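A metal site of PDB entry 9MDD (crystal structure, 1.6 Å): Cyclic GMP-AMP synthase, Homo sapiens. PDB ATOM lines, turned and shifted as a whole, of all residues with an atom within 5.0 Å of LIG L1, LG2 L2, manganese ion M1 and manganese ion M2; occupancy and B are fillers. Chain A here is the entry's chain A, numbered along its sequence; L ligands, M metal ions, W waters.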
ATOM      1  N   THR A  55      -9.401  10.938   8.216  1.00  0.00           N
ATOM      2  CA  THR A  55      -9.342  11.781   7.032  1.00  0.00           C
ATOM      3  C   THR A  55      -8.007  11.586   6.330  1.00  0.00           C
ATOM      4  O   THR A  55      -7.128  10.871   6.809  1.00  0.00           O
ATOM      5  CB  THR A  55      -9.600  13.235   7.447  1.00  0.00           C
ATOM      6  OG1 THR A  55     -10.139  13.969   6.354  1.00  0.00           O
ATOM      7  CG2 THR A  55      -8.328  13.895   7.963  1.00  0.00           C
ATOM      8  N   GLY A  56      -7.849  12.226   5.156  1.00  0.00           N
ATOM      9  CA  GLY A  56      -6.577  12.158   4.472  1.00  0.00           C
ATOM     10  C   GLY A  56      -6.400  10.900   3.631  1.00  0.00           C
ATOM     11  O   GLY A  56      -7.300  10.066   3.475  1.00  0.00           O
ATOM     12  N   SER A  57      -5.185  10.761   3.096  1.00  0.00           N
ATOM     13  CA  SER A  57      -5.009   9.874   1.940  1.00  0.00           C
ATOM     14  C   SER A  57      -5.242   8.401   2.261  1.00  0.00           C
ATOM     15  O   SER A  57      -5.701   7.652   1.402  1.00  0.00           O
ATOM     16  CB  SER A  57      -3.617  10.062   1.338  1.00  0.00           C
ATOM     17  OG  SER A  57      -2.593   9.554   2.190  1.00  0.00           O
ATOM     18  N   GLU A  60      -8.862   7.928   1.949  1.00  0.00           N
ATOM     19  CA  GLU A  60      -9.234   8.216   0.562  1.00  0.00           C
ATOM     20  C   GLU A  60      -8.741   7.148  -0.384  1.00  0.00           C
ATOM     21  O   GLU A  60      -9.054   7.213  -1.578  1.00  0.00           O
ATOM     22  CB  GLU A  60      -8.654   9.560   0.117  1.00  0.00           C
ATOM     23  CG  GLU A  60      -9.230  10.767   0.862  1.00  0.00           C
ATOM     24  CD  GLU A  60      -8.389  12.018   0.707  1.00  0.00           C
ATOM     25  OE1 GLU A  60      -7.212  11.955   0.286  1.00  0.00           O
ATOM     26  OE2 GLU A  60      -8.935  13.105   1.016  1.00  0.00           O
ATOM     27  N   VAL A  62      -5.742   6.767  -1.468  1.00  0.00           N
ATOM     28  CA  VAL A  62      -4.697   7.267  -2.370  1.00  0.00           C
ATOM     29  C   VAL A  62      -3.378   7.438  -1.603  1.00  0.00           C
ATOM     30  O   VAL A  62      -2.461   8.135  -2.066  1.00  0.00           O
ATOM     31  CB  VAL A  62      -5.111   8.581  -3.070  1.00  0.00           C
ATOM     32  CG1 VAL A  62      -6.290   8.325  -4.017  1.00  0.00           C
ATOM     33  CG2 VAL A  62      -5.452   9.688  -2.059  1.00  0.00           C
ATOM     34  N   LYS A  63      -3.246   6.760  -0.464  1.00  0.00           N
ATOM     35  CA  LYS A  63      -1.943   6.641   0.169  1.00  0.00           C
ATOM     36  C   LYS A  63      -1.064   5.710  -0.677  1.00  0.00           C
ATOM     37  O   LYS A  63      -1.501   4.624  -1.060  1.00  0.00           O
ATOM     38  CB  LYS A  63      -2.096   6.079   1.586  1.00  0.00           C
ATOM     39  CG  LYS A  63      -0.750   5.882   2.312  1.00  0.00           C
ATOM     40  CD  LYS A  63      -0.278   7.178   2.959  1.00  0.00           C
ATOM     41  CE  LYS A  63       1.130   7.086   3.520  1.00  0.00           C
ATOM     42  NZ  LYS A  63       2.207   6.941   2.495  1.00  0.00           N
ATOM     43  N   GLU A  69       1.498   6.776   7.261  1.00  0.00           N
ATOM     44  CA  GLU A  69       1.106   8.142   7.642  1.00  0.00           C
ATOM     45  C   GLU A  69      -0.414   8.237   7.630  1.00  0.00           C
ATOM     46  O   GLU A  69      -1.075   8.040   6.600  1.00  0.00           O
ATOM     47  CB  GLU A  69       1.722   9.179   6.695  1.00  0.00           C
ATOM     48  CG  GLU A  69       1.874  10.586   7.360  1.00  0.00           C
ATOM     49  CD  GLU A  69       0.692  11.518   7.127  1.00  0.00           C
ATOM     50  OE1 GLU A  69      -0.292  11.084   6.516  1.00  0.00           O
ATOM     51  OE2 GLU A  69       0.786  12.700   7.569  1.00  0.00           O
ATOM     52  N   PHE A  70      -0.985   8.493   8.807  1.00  0.00           N
ATOM     53  CA  PHE A  70      -2.415   8.546   8.999  1.00  0.00           C
ATOM     54  C   PHE A  70      -2.812   9.915   9.543  1.00  0.00           C
ATOM     55  O   PHE A  70      -2.070  10.489  10.341  1.00  0.00           O
ATOM     56  CB  PHE A  70      -2.881   7.512  10.018  1.00  0.00           C
ATOM     57  CG  PHE A  70      -2.703   6.080   9.578  1.00  0.00           C
ATOM     58  CD1 PHE A  70      -1.438   5.498   9.594  1.00  0.00           C
ATOM     59  CD2 PHE A  70      -3.794   5.313   9.178  1.00  0.00           C
ATOM     60  CE1 PHE A  70      -1.263   4.189   9.223  1.00  0.00           C
ATOM     61  CE2 PHE A  70      -3.617   3.989   8.811  1.00  0.00           C
ATOM     62  CZ  PHE A  70      -2.335   3.433   8.834  1.00  0.00           C
ATOM     63  N   ASP A  71      -4.013  10.369   9.180  1.00  0.00           N
ATOM     64  CA  ASP A  71      -4.559  11.634   9.652  1.00  0.00           C
ATOM     65  C   ASP A  71      -5.903  11.402  10.329  1.00  0.00           C
ATOM     66  O   ASP A  71      -6.742  10.694   9.789  1.00  0.00           O
ATOM     67  CB  ASP A  71      -4.720  12.599   8.476  1.00  0.00           C
ATOM     68  CG  ASP A  71      -3.423  12.801   7.747  1.00  0.00           C
ATOM     69  OD1 ASP A  71      -2.514  13.455   8.306  1.00  0.00           O
ATOM     70  OD2 ASP A  71      -3.303  12.239   6.615  1.00  0.00           O
ATOM     71  N   MET A  73      -8.947  13.586  12.758  1.00  0.00           N
ATOM     72  CA  MET A  73      -9.442  14.787  13.422  1.00  0.00           C
ATOM     73  C   MET A  73     -10.072  14.375  14.745  1.00  0.00           C
ATOM     74  O   MET A  73     -10.855  13.415  14.793  1.00  0.00           O
ATOM     75  CB  MET A  73     -10.468  15.458  12.520  1.00  0.00           C
ATOM     76  CG  MET A  73      -9.857  15.740  11.147  1.00  0.00           C
ATOM     77  SD  MET A  73     -11.049  16.447  10.010  1.00  0.00           S
ATOM     78  CE  MET A  73     -11.331  18.002  10.833  1.00  0.00           C
ATOM     79  N   ARG A 146       5.927  20.739  14.311  1.00  0.00           N
ATOM     80  CA  ARG A 146       6.145  20.943  12.887  1.00  0.00           C
ATOM     81  C   ARG A 146       5.548  22.300  12.544  1.00  0.00           C
ATOM     82  O   ARG A 146       4.327  22.486  12.628  1.00  0.00           O
ATOM     83  CB  ARG A 146       5.488  19.807  12.092  1.00  0.00           C
ATOM     84  CG  ARG A 146       5.666  19.807  10.578  1.00  0.00           C
ATOM     85  CD  ARG A 146       5.188  18.469   9.978  1.00  0.00           C
ATOM     86  NE  ARG A 146       3.765  18.262  10.178  1.00  0.00           N
ATOM     87  CZ  ARG A 146       3.147  17.084  10.238  1.00  0.00           C
ATOM     88  NH1 ARG A 146       3.817  15.944  10.172  1.00  0.00           N
ATOM     89  NH2 ARG A 146       1.829  17.045  10.381  1.00  0.00           N
ATOM     90  N   GLY A 148       3.701  25.526  11.539  1.00  0.00           N
ATOM     91  CA  GLY A 148       2.458  25.694  10.823  1.00  0.00           C
ATOM     92  C   GLY A 148       1.565  24.468  10.771  1.00  0.00           C
ATOM     93  O   GLY A 148       0.666  24.383   9.934  1.00  0.00           O
ATOM     94  N   SER A 149       1.804  23.507  11.628  1.00  0.00           N
ATOM     95  CA  SER A 149       0.919  22.353  11.606  1.00  0.00           C
ATOM     96  C   SER A 149      -0.149  22.507  12.671  1.00  0.00           C
ATOM     97  O   SER A 149       0.191  22.849  13.815  1.00  0.00           O
ATOM     98  CB  SER A 149       1.710  21.066  11.860  1.00  0.00           C
ATOM     99  OG  SER A 149       0.848  19.980  12.125  1.00  0.00           O
ATOM    100  N   PRO A 150      -1.425  22.273  12.363  1.00  0.00           N
ATOM    101  CA  PRO A 150      -2.437  22.229  13.421  1.00  0.00           C
ATOM    102  C   PRO A 150      -2.471  20.900  14.164  1.00  0.00           C
ATOM    103  O   PRO A 150      -3.295  20.736  15.055  1.00  0.00           O
ATOM    104  CB  PRO A 150      -3.747  22.446  12.666  1.00  0.00           C
ATOM    105  CG  PRO A 150      -3.495  21.830  11.326  1.00  0.00           C
ATOM    106  CD  PRO A 150      -2.007  22.005  11.039  1.00  0.00           C
ATOM    107  N   ASP A 163      -1.050  11.979  12.506  1.00  0.00           N
ATOM    108  CA  ASP A 163      -1.320  13.393  12.763  1.00  0.00           C
ATOM    109  C   ASP A 163      -2.706  13.519  13.368  1.00  0.00           C
ATOM    110  O   ASP A 163      -3.696  13.237  12.688  1.00  0.00           O
ATOM    111  CB  ASP A 163      -1.263  14.219  11.489  1.00  0.00           C
ATOM    112  CG  ASP A 163       0.116  14.318  10.923  1.00  0.00           C
ATOM    113  OD1 ASP A 163       1.097  14.345  11.680  1.00  0.00           O
ATOM    114  OD2 ASP A 163       0.222  14.458   9.681  1.00  0.00           O
ATOM    115  N   THR A 165      -5.402  16.048  14.704  1.00  0.00           N
ATOM    116  CA  THR A 165      -5.744  17.464  14.580  1.00  0.00           C
ATOM    117  C   THR A 165      -6.998  17.769  15.387  1.00  0.00           C
ATOM    118  O   THR A 165      -8.076  17.241  15.088  1.00  0.00           O
ATOM    119  CB  THR A 165      -5.927  17.851  13.108  1.00  0.00           C
ATOM    120  OG1 THR A 165      -4.718  17.589  12.400  1.00  0.00           O
ATOM    121  CG2 THR A 165      -6.276  19.334  12.961  1.00  0.00           C
ATOM    122  N   VAL A 204      -9.506  24.409  12.501  1.00  0.00           N
ATOM    123  CA  VAL A 204      -8.332  23.763  13.081  1.00  0.00           C
ATOM    124  C   VAL A 204      -7.357  24.843  13.550  1.00  0.00           C
ATOM    125  O   VAL A 204      -7.412  25.981  13.066  1.00  0.00           O
ATOM    126  CB  VAL A 204      -7.667  22.798  12.078  1.00  0.00           C
ATOM    127  CG1 VAL A 204      -8.669  21.707  11.679  1.00  0.00           C
ATOM    128  CG2 VAL A 204      -7.115  23.545  10.847  1.00  0.00           C
ATOM    129  N   LYS A 206      -4.594  26.308  13.089  1.00  0.00           N
ATOM    130  CA  LYS A 206      -3.529  26.824  12.248  1.00  0.00           C
ATOM    131  C   LYS A 206      -3.721  28.328  12.150  1.00  0.00           C
ATOM    132  O   LYS A 206      -4.822  28.797  11.839  1.00  0.00           O
ATOM    133  CB  LYS A 206      -3.538  26.153  10.862  1.00  0.00           C
ATOM    134  CG  LYS A 206      -2.548  26.743   9.895  1.00  0.00           C
ATOM    135  CD  LYS A 206      -2.366  25.823   8.715  1.00  0.00           C
ATOM    136  CE  LYS A 206      -1.641  26.560   7.622  1.00  0.00           C
ATOM    137  NZ  LYS A 206      -0.243  26.063   7.620  1.00  0.00           N
ATOM    138  N   ARG A 220      -8.299  28.109  11.350  1.00  0.00           N
ATOM    139  CA  ARG A 220      -8.387  28.004   9.900  1.00  0.00           C
ATOM    140  C   ARG A 220      -9.451  27.000   9.497  1.00  0.00           C
ATOM    141  O   ARG A 220      -9.614  25.955  10.139  1.00  0.00           O
ATOM    142  CB  ARG A 220      -7.040  27.592   9.301  1.00  0.00           C
ATOM    143  CG  ARG A 220      -7.074  27.527   7.769  1.00  0.00           C
ATOM    144  CD  ARG A 220      -5.752  27.843   7.124  1.00  0.00           C
ATOM    145  NE  ARG A 220      -5.676  27.238   5.799  1.00  0.00           N
ATOM    146  CZ  ARG A 220      -4.640  27.331   4.971  1.00  0.00           C
ATOM    147  NH1 ARG A 220      -3.586  28.080   5.266  1.00  0.00           N
ATOM    148  NH2 ARG A 220      -4.645  26.638   3.836  1.00  0.00           N
ATOM    149  N   LEU A 221     -10.172  27.317   8.425  1.00  0.00           N
ATOM    150  CA  LEU A 221     -11.186  26.405   7.909  1.00  0.00           C
ATOM    151  C   LEU A 221     -10.525  25.136   7.382  1.00  0.00           C
ATOM    152  O   LEU A 221      -9.474  25.181   6.740  1.00  0.00           O
ATOM    153  CB  LEU A 221     -11.932  27.106   6.773  1.00  0.00           C
ATOM    154  CG  LEU A 221     -13.095  28.008   7.174  1.00  0.00           C
ATOM    155  CD1 LEU A 221     -13.745  28.627   5.933  1.00  0.00           C
ATOM    156  CD2 LEU A 221     -14.129  27.306   8.043  1.00  0.00           C
ATOM    157  N   SER A 222     -11.154  23.981   7.641  1.00  0.00           N
ATOM    158  CA  SER A 222     -10.736  22.741   7.004  1.00  0.00           C
ATOM    159  C   SER A 222     -11.946  22.029   6.445  1.00  0.00           C
ATOM    160  O   SER A 222     -12.967  21.901   7.127  1.00  0.00           O
ATOM    161  CB  SER A 222      -9.995  21.829   7.994  1.00  0.00           C
ATOM    162  OG  SER A 222      -9.648  20.592   7.346  1.00  0.00           O
ATOM    163  N   SER A 224     -11.304  18.873   4.991  1.00  0.00           N
ATOM    164  CA  SER A 224     -10.693  17.575   4.751  1.00  0.00           C
ATOM    165  C   SER A 224     -11.759  16.493   4.648  1.00  0.00           C
ATOM    166  O   SER A 224     -11.622  15.550   3.846  1.00  0.00           O
ATOM    167  CB  SER A 224      -9.696  17.249   5.872  1.00  0.00           C
ATOM    168  OG  SER A 224      -8.900  16.120   5.565  1.00  0.00           O
ATOM    169  N   GLU A 227     -13.298  16.566   1.138  1.00  0.00           N
ATOM    170  CA  GLU A 227     -12.344  16.003   0.194  1.00  0.00           C
ATOM    171  C   GLU A 227     -12.432  14.481   0.185  1.00  0.00           C
ATOM    172  O   GLU A 227     -12.396  13.849  -0.884  1.00  0.00           O
ATOM    173  CB  GLU A 227     -10.934  16.455   0.572  1.00  0.00           C
ATOM    174  CG  GLU A 227     -10.795  17.965   0.457  1.00  0.00           C
ATOM    175  CD  GLU A 227      -9.546  18.514   1.124  1.00  0.00           C
ATOM    176  OE1 GLU A 227      -8.659  17.710   1.518  1.00  0.00           O
ATOM    177  OE2 GLU A 227      -9.490  19.756   1.313  1.00  0.00           O
ATOM    178  N   LYS A 258       1.062  12.675  -6.828  1.00  0.00           N
ATOM    179  CA  LYS A 258       1.641  12.692  -5.489  1.00  0.00           C
ATOM    180  C   LYS A 258       3.037  12.109  -5.485  1.00  0.00           C
ATOM    181  O   LYS A 258       3.930  12.632  -4.811  1.00  0.00           O
ATOM    182  CB  LYS A 258       0.742  11.918  -4.516  1.00  0.00           C
ATOM    183  CG  LYS A 258      -0.553  12.639  -4.182  1.00  0.00           C
ATOM    184  CD  LYS A 258      -1.470  11.780  -3.330  1.00  0.00           C
ATOM    185  CE  LYS A 258      -0.911  11.706  -1.894  1.00  0.00           C
ATOM    186  NZ  LYS A 258      -1.737  10.826  -1.056  1.00  0.00           N
ATOM    187  N   SER A 278       3.497  20.781  -0.955  1.00  0.00           N
ATOM    188  CA  SER A 278       3.032  19.594  -0.267  1.00  0.00           C
ATOM    189  C   SER A 278       2.042  18.853  -1.140  1.00  0.00           C
ATOM    190  O   SER A 278       1.612  19.337  -2.202  1.00  0.00           O
ATOM    191  CB  SER A 278       2.361  19.916   1.079  1.00  0.00           C
ATOM    192  OG  SER A 278       1.046  20.383   0.882  1.00  0.00           O
ATOM    193  N   SER A 279       1.645  17.672  -0.680  1.00  0.00           N
ATOM    194  CA  SER A 279       0.702  16.910  -1.501  1.00  0.00           C
ATOM    195  C   SER A 279      -0.641  17.621  -1.623  1.00  0.00           C
ATOM    196  O   SER A 279      -1.427  17.278  -2.511  1.00  0.00           O
ATOM    197  CB  SER A 279       0.516  15.509  -0.920  1.00  0.00           C
ATOM    198  OG  SER A 279       0.035  15.567   0.409  1.00  0.00           O
ATOM    199  N   TYR A 280      -0.954  18.593  -0.758  1.00  0.00           N
ATOM    200  CA  TYR A 280      -2.214  19.312  -0.922  1.00  0.00           C
ATOM    201  C   TYR A 280      -2.205  20.190  -2.160  1.00  0.00           C
ATOM    202  O   TYR A 280      -3.269  20.458  -2.736  1.00  0.00           O
ATOM    203  CB  TYR A 280      -2.522  20.156   0.317  1.00  0.00           C
ATOM    204  CG  TYR A 280      -3.974  20.583   0.365  1.00  0.00           C
ATOM    205  CD1 TYR A 280      -4.989  19.651   0.581  1.00  0.00           C
ATOM    206  CD2 TYR A 280      -4.327  21.926   0.171  1.00  0.00           C
ATOM    207  CE1 TYR A 280      -6.315  20.028   0.595  1.00  0.00           C
ATOM    208  CE2 TYR A 280      -5.662  22.299   0.205  1.00  0.00           C
ATOM    209  CZ  TYR A 280      -6.652  21.347   0.418  1.00  0.00           C
ATOM    210  OH  TYR A 280      -7.960  21.749   0.439  1.00  0.00           O
ATOM    211  N   LYS A 283      -3.198  17.742  -4.771  1.00  0.00           N
ATOM    212  CA  LYS A 283      -4.588  17.372  -4.536  1.00  0.00           C
ATOM    213  C   LYS A 283      -5.541  18.462  -5.023  1.00  0.00           C
ATOM    214  O   LYS A 283      -6.561  18.168  -5.675  1.00  0.00           O
ATOM    215  CB  LYS A 283      -4.816  17.078  -3.046  1.00  0.00           C
ATOM    216  CG  LYS A 283      -6.114  16.350  -2.732  1.00  0.00           C
ATOM    217  CD  LYS A 283      -6.233  16.204  -1.183  1.00  0.00           C
ATOM    218  CE  LYS A 283      -7.356  15.282  -0.778  1.00  0.00           C
ATOM    219  NZ  LYS A 283      -7.541  15.286   0.724  1.00  0.00           N
ATOM    220  N   ASN A 326      -7.710  27.635  -3.731  1.00  0.00           N
ATOM    221  CA  ASN A 326      -8.247  26.608  -2.857  1.00  0.00           C
ATOM    222  C   ASN A 326      -9.610  26.157  -3.403  1.00  0.00           C
ATOM    223  O   ASN A 326     -10.411  26.966  -3.859  1.00  0.00           O
ATOM    224  CB  ASN A 326      -8.355  27.169  -1.446  1.00  0.00           C
ATOM    225  CG  ASN A 326      -8.908  26.163  -0.454  1.00  0.00           C
ATOM    226  OD1 ASN A 326     -10.110  25.897  -0.428  1.00  0.00           O
ATOM    227  ND2 ASN A 326      -8.025  25.599   0.377  1.00  0.00           N
HETATM  228  C1  LIG L   1      -0.740  22.110   7.059  1.00  0.00           C
HETATM  229  C2  LIG L   1      -3.929  20.267   7.880  1.00  0.00           C
HETATM  230  C3  LIG L   1      -5.914  21.631   7.734  1.00  0.00           C
HETATM  231  C4  LIG L   1      -3.718  22.527   7.154  1.00  0.00           C
HETATM  232  C5  LIG L   1      -6.743  17.349   9.311  1.00  0.00           C
HETATM  233  C6  LIG L   1      -7.843  18.079   8.922  1.00  0.00           C
HETATM  234  C7  LIG L   1       0.719  19.835   5.361  1.00  0.00           C
HETATM  235  C8  LIG L   1      -0.731  17.276   7.818  1.00  0.00           C
HETATM  236  C9  LIG L   1       2.235  15.385   6.607  1.00  0.00           C
HETATM  237  C10 LIG L   1       0.712  17.001   7.340  1.00  0.00           C
HETATM  238  C11 LIG L   1       1.705  18.032   7.195  1.00  0.00           C
HETATM  239  C12 LIG L   1       2.954  17.643   6.732  1.00  0.00           C
HETATM  240  C13 LIG L   1       3.251  16.332   6.430  1.00  0.00           C
HETATM  241  C14 LIG L   1       1.433  19.430   7.556  1.00  0.00           C
HETATM  242  C15 LIG L   1       0.750  21.747   6.912  1.00  0.00           C
HETATM  243  C16 LIG L   1      -3.101  21.316   7.453  1.00  0.00           C
HETATM  244  C17 LIG L   1      -5.300  20.436   8.039  1.00  0.00           C
HETATM  245  C18 LIG L   1      -5.086  22.629   7.305  1.00  0.00           C
HETATM  246  C19 LIG L   1      -6.139  19.345   8.483  1.00  0.00           C
HETATM  247  C20 LIG L   1       1.235  22.685   5.841  1.00  0.00           C
HETATM  248  N1  LIG L   1       1.012  15.725   7.032  1.00  0.00           N
HETATM  249  N2  LIG L   1       0.980  20.348   6.606  1.00  0.00           N
HETATM  250  N3  LIG L   1      -1.704  21.103   7.306  1.00  0.00           N
HETATM  251  N4  LIG L   1      -5.650  18.167   9.055  1.00  0.00           N
HETATM  252  N5  LIG L   1      -7.469  19.311   8.408  1.00  0.00           N
HETATM  253  O1  LIG L   1      -1.057  23.263   6.915  1.00  0.00           O
HETATM  254  O2  LIG L   1       1.659  19.806   8.647  1.00  0.00           O
HETATM  255  O3  LIG L   1      -1.072  18.465   7.900  1.00  0.00           O
HETATM  256  O4  LIG L   1      -1.391  16.259   8.058  1.00  0.00           O
HETATM  257 CL1  LIG L   1      -5.846  24.161   6.917  1.00  0.00          CL
HETATM  258  P1  LG2 L   2      -0.298  12.123   2.034  1.00  0.00           P
HETATM  259  O1  LG2 L   2      -0.322  11.911   3.527  1.00  0.00           O
HETATM  260  O2  LG2 L   2      -0.462  10.761   1.349  1.00  0.00           O
HETATM  261  O3  LG2 L   2       1.040  12.807   1.550  1.00  0.00           O
HETATM  262  P2  LG2 L   2      -2.759  13.669   2.568  1.00  0.00           P
HETATM  263  O4  LG2 L   2      -3.913  14.154   1.754  1.00  0.00           O
HETATM  264  O5  LG2 L   2      -3.143  12.654   3.666  1.00  0.00           O
HETATM  265  N1  LG2 L   2      -1.588  13.080   1.515  1.00  0.00           N
HETATM  266  P3  LG2 L   2      -1.535  15.373   4.630  1.00  0.00           P
HETATM  267  O6  LG2 L   2      -0.397  16.295   4.361  1.00  0.00           O
HETATM  268  O7  LG2 L   2      -1.213  14.175   5.562  1.00  0.00           O
HETATM  269  O8  LG2 L   2      -2.120  14.959   3.198  1.00  0.00           O
HETATM  270  O9  LG2 L   2      -2.695  16.251   5.231  1.00  0.00           O
HETATM  271  C1  LG2 L   2      -3.886  15.658   5.760  1.00  0.00           C
HETATM  272  C2  LG2 L   2      -5.080  16.467   5.281  1.00  0.00           C
HETATM  273  O10 LG2 L   2      -4.982  17.804   5.808  1.00  0.00           O
HETATM  274  C3  LG2 L   2      -5.197  16.673   3.770  1.00  0.00           C
HETATM  275  O11 LG2 L   2      -5.808  15.573   3.097  1.00  0.00           O
HETATM  276  C4  LG2 L   2      -6.062  17.929   3.695  1.00  0.00           C
HETATM  277  O12 LG2 L   2      -7.456  17.641   3.802  1.00  0.00           O
HETATM  278  C5  LG2 L   2      -5.569  18.729   4.899  1.00  0.00           C
HETATM  279  N2  LG2 L   2      -4.563  19.705   4.509  1.00  0.00           N
HETATM  280  C6  LG2 L   2      -3.213  19.517   4.372  1.00  0.00           C
HETATM  281  N3  LG2 L   2      -2.575  20.560   3.919  1.00  0.00           N
HETATM  282  C7  LG2 L   2      -3.566  21.514   3.750  1.00  0.00           C
HETATM  283  C8  LG2 L   2      -3.537  22.843   3.303  1.00  0.00           C
HETATM  284  N4  LG2 L   2      -2.426  23.484   2.918  1.00  0.00           N
HETATM  285  N5  LG2 L   2      -4.715  23.506   3.244  1.00  0.00           N
HETATM  286  C9  LG2 L   2      -5.837  22.871   3.595  1.00  0.00           C
HETATM  287  N6  LG2 L   2      -5.984  21.620   4.031  1.00  0.00           N
HETATM  288  C10 LG2 L   2      -4.803  20.993   4.085  1.00  0.00           C
HETATM  289 MN    MN M   1      -0.593  14.273   7.713  1.00  0.00          MN
HETATM  290 MN    MN M   2      -1.704  12.037   5.180  1.00  0.00          MN
HETATM  291  O   HOH W   1       1.792  14.913   3.031  1.00  0.00           O
HETATM  292  O   HOH W   2      -0.668  17.971   2.198  1.00  0.00           O
HETATM  293  O   HOH W   3      -5.217  25.586   1.169  1.00  0.00           O
HETATM  294  O   HOH W   4      -3.077  17.087   9.806  1.00  0.00           O
HETATM  295  O   HOH W   5      -4.693  12.742  -0.413  1.00  0.00           O
HETATM  296  O   HOH W   6       1.169   8.844   0.287  1.00  0.00           O
HETATM  297  O   HOH W   7      -2.909  16.611   0.568  1.00  0.00           O
HETATM  298  O   HOH W   8      -2.057  26.607   1.624  1.00  0.00           O
HETATM  299  O   HOH W   9      -2.401   9.823   4.866  1.00  0.00           O
HETATM  300  O   HOH W  10      -4.840  15.190  11.040  1.00  0.00           O
HETATM  301  O   HOH W  11       2.328  11.353   4.223  1.00  0.00           O
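The side-chain hydroxyl of Ser 279 is in hydrogen-bond range of an oxygen (O3) of LG2 L2. An oxygen (O2) of LIG L1 sits at hydrogen-bond distance from the guanidinium group (NE) of Arg 146, at 3.0 Å. The side-chain hydroxyl (OG) of Ser 222 is in hydrogen-bond range of a nitrogen (N5) of LIG L1, at 2.7 Å. An oxygen (O4) of LG2 L2 is in salt-bridge range of the side-chain amino group of Lys 283, at 3.9 Å. The side-chain carboxylate (OE1) of Glu 227 is in hydrogen-bond range of an oxygen (O12) of LG2 L2, at 2.6 Å. An oxygen (O2) of LG2 L2 lies within salt-bridge range of the side-chain amino group (NZ) of Lys 258, 2.7 Å away. N of Ser 57 sits close to O5 of LG2 L2, at 2.8 Å. OG of Ser 57 is in hydrogen-bond range of O2 of LG2 L2 (2.6 Å). NZ of Lys 206 lies within hydrogen-bond range of O1 of LIG L1, 3.0 Å away. A nitrogen (N5) of LG2 L2 is in hydrogen-bond range of the guanidinium group (NH2) of Arg 220 (3.2 Å). The side-chain hydroxyl (OG) of Ser 224 sits at hydrogen-bond distance from an oxygen (O12) of LG2 L2 (2.7 Å).
The backbone NH (N) of Tyr 280 sits close to the side-chain hydroxyl (OG) of Ser 278, at 3.1 Å. OE1 of Glu 227 is in salt-bridge range of NZ of Lys 283 (2.8 Å). The backbone NH of Ser 224 sits at hydrogen-bond distance from the side-chain hydroxyl of Ser 222. The side-chain amino group (NZ) of Lys 258 lies within hydrogen-bond range of the backbone carbonyl oxygen (O) of Val 62 (3.0 Å). N of Thr 55 is in hydrogen-bond range of O of Asp 71. The backbone NH of Asp 163 is in hydrogen-bond range of the backbone carbonyl oxygen of Phe 70, 2.8 Å away. N of Lys 63 lies within hydrogen-bond range of O of Ser 57, 3.2 Å away. OE2 of Glu 227 sits at hydrogen-bond distance from OH of Tyr 280, 2.7 Å away.
Residues that only touch LIG L1: Met 73 (3.8 Å), Gly 148 (3.7 Å), Ser 149 (3.5 Å), Pro 150 (3.8 Å), Thr 165 (3.5 Å), Val 204 (3.8 Å), Arg 220 (3.3 Å), Leu 221 (3.8 Å) and Ser 224 (3.7 Å). Hydrophobic or aromatic side chains that line LIG L1: Met 73, Pro 150 and Val 204. Along chain A the residues within 4 Å of LIG L1 span positions 69 to 224. The nearest printed residue that does not touch LIG L1 is Thr 55 (4.03 Å).
Gly 56 touches LG2 L2 (CA to O5, 3.6 Å). CD of Lys 63 touches O2 of LG2 L2, 3.9 Å away. Tyr 280 touches LG2 L2 (CD2 to C8, 3.4 Å). Hydrophobic or aromatic side chains within 4 Å of LG2 L2: Tyr 280. 12 residues have an atom within 4 Å of LG2 L2: Gly 56, Ser 57, Lys 63, Glu 69, Asp 71, Arg 220, Ser 224, Glu 227, Lys 258, Ser 279, Tyr 280 and Lys 283. The nearest printed residue that does not touch LG2 L2 is Glu 60 (4.2 Å).
The nearest printed residue that does not touch manganese ion M1 is Arg 146 (4.5 Å).
OG of Ser 57 touches manganese ion M2 (3.99 Å). Three residues have an atom within 4 Å of manganese ion M2: Ser 57, Glu 69 and Asp 71.
Manganese ion M1 is bound by the side-chain carboxylate of Glu 69 (2.1 Å), the side-chain carboxylate of Asp 163 (2.1 Å), an oxygen (O4) of LIG L1 (2.2 Å), the side-chain carboxylate of Asp 71 (2.2 Å), an oxygen (O7) of LG2 L2 (2.2 Å) and a nitrogen (N1) of LIG L1 (2.3 Å).
OD2 of Asp 71 is bound to manganese ion M2 (2.2 Å). O1 of LG2 L2 binds manganese ion M2, 2.2 Å away. The side-chain carboxylate (OE1) of Glu 69 is bound to manganese ion M2. O5 of LG2 L2 binds manganese ion M2, at 2.2 Å. O7 of LG2 L2 is bound to manganese ion M2 (2.2 Å). Manganese ion M2 is bound by water W9 (2.3 Å).
Water W1 lies within hydrogen-bond range of O3 of LG2 L2 and OG of Ser 279. Water W6 lies within hydrogen-bond range of O2 of LG2 L2 (2.7 Å) and NZ of Lys 63 (3.1 Å). Water W2 lies within hydrogen-bond range of O6 of LG2 L2 (2.7 Å), N of Tyr 280 (3.0 Å), OG of Ser 279 (3.1 Å) and OG of Ser 278 (3.2 Å). Water W7 lies within hydrogen-bond range of an oxygen (O4) of LG2 L2 (2.9 Å), the backbone NH (N) of Tyr 280 (3.1 Å) and the side-chain hydroxyl (OG) of Ser 279 (3.1 Å). Water W3 lies within hydrogen-bond range of the side-chain amide nitrogen (ND2) of Asn 326 (2.9 Å), the guanidinium group (NH2) of Arg 220 (2.9 Å) and a nitrogen (N5) of LG2 L2 (3.0 Å). Water W8 bridges N4 of LG2 L2 and NH2 of Arg 220.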
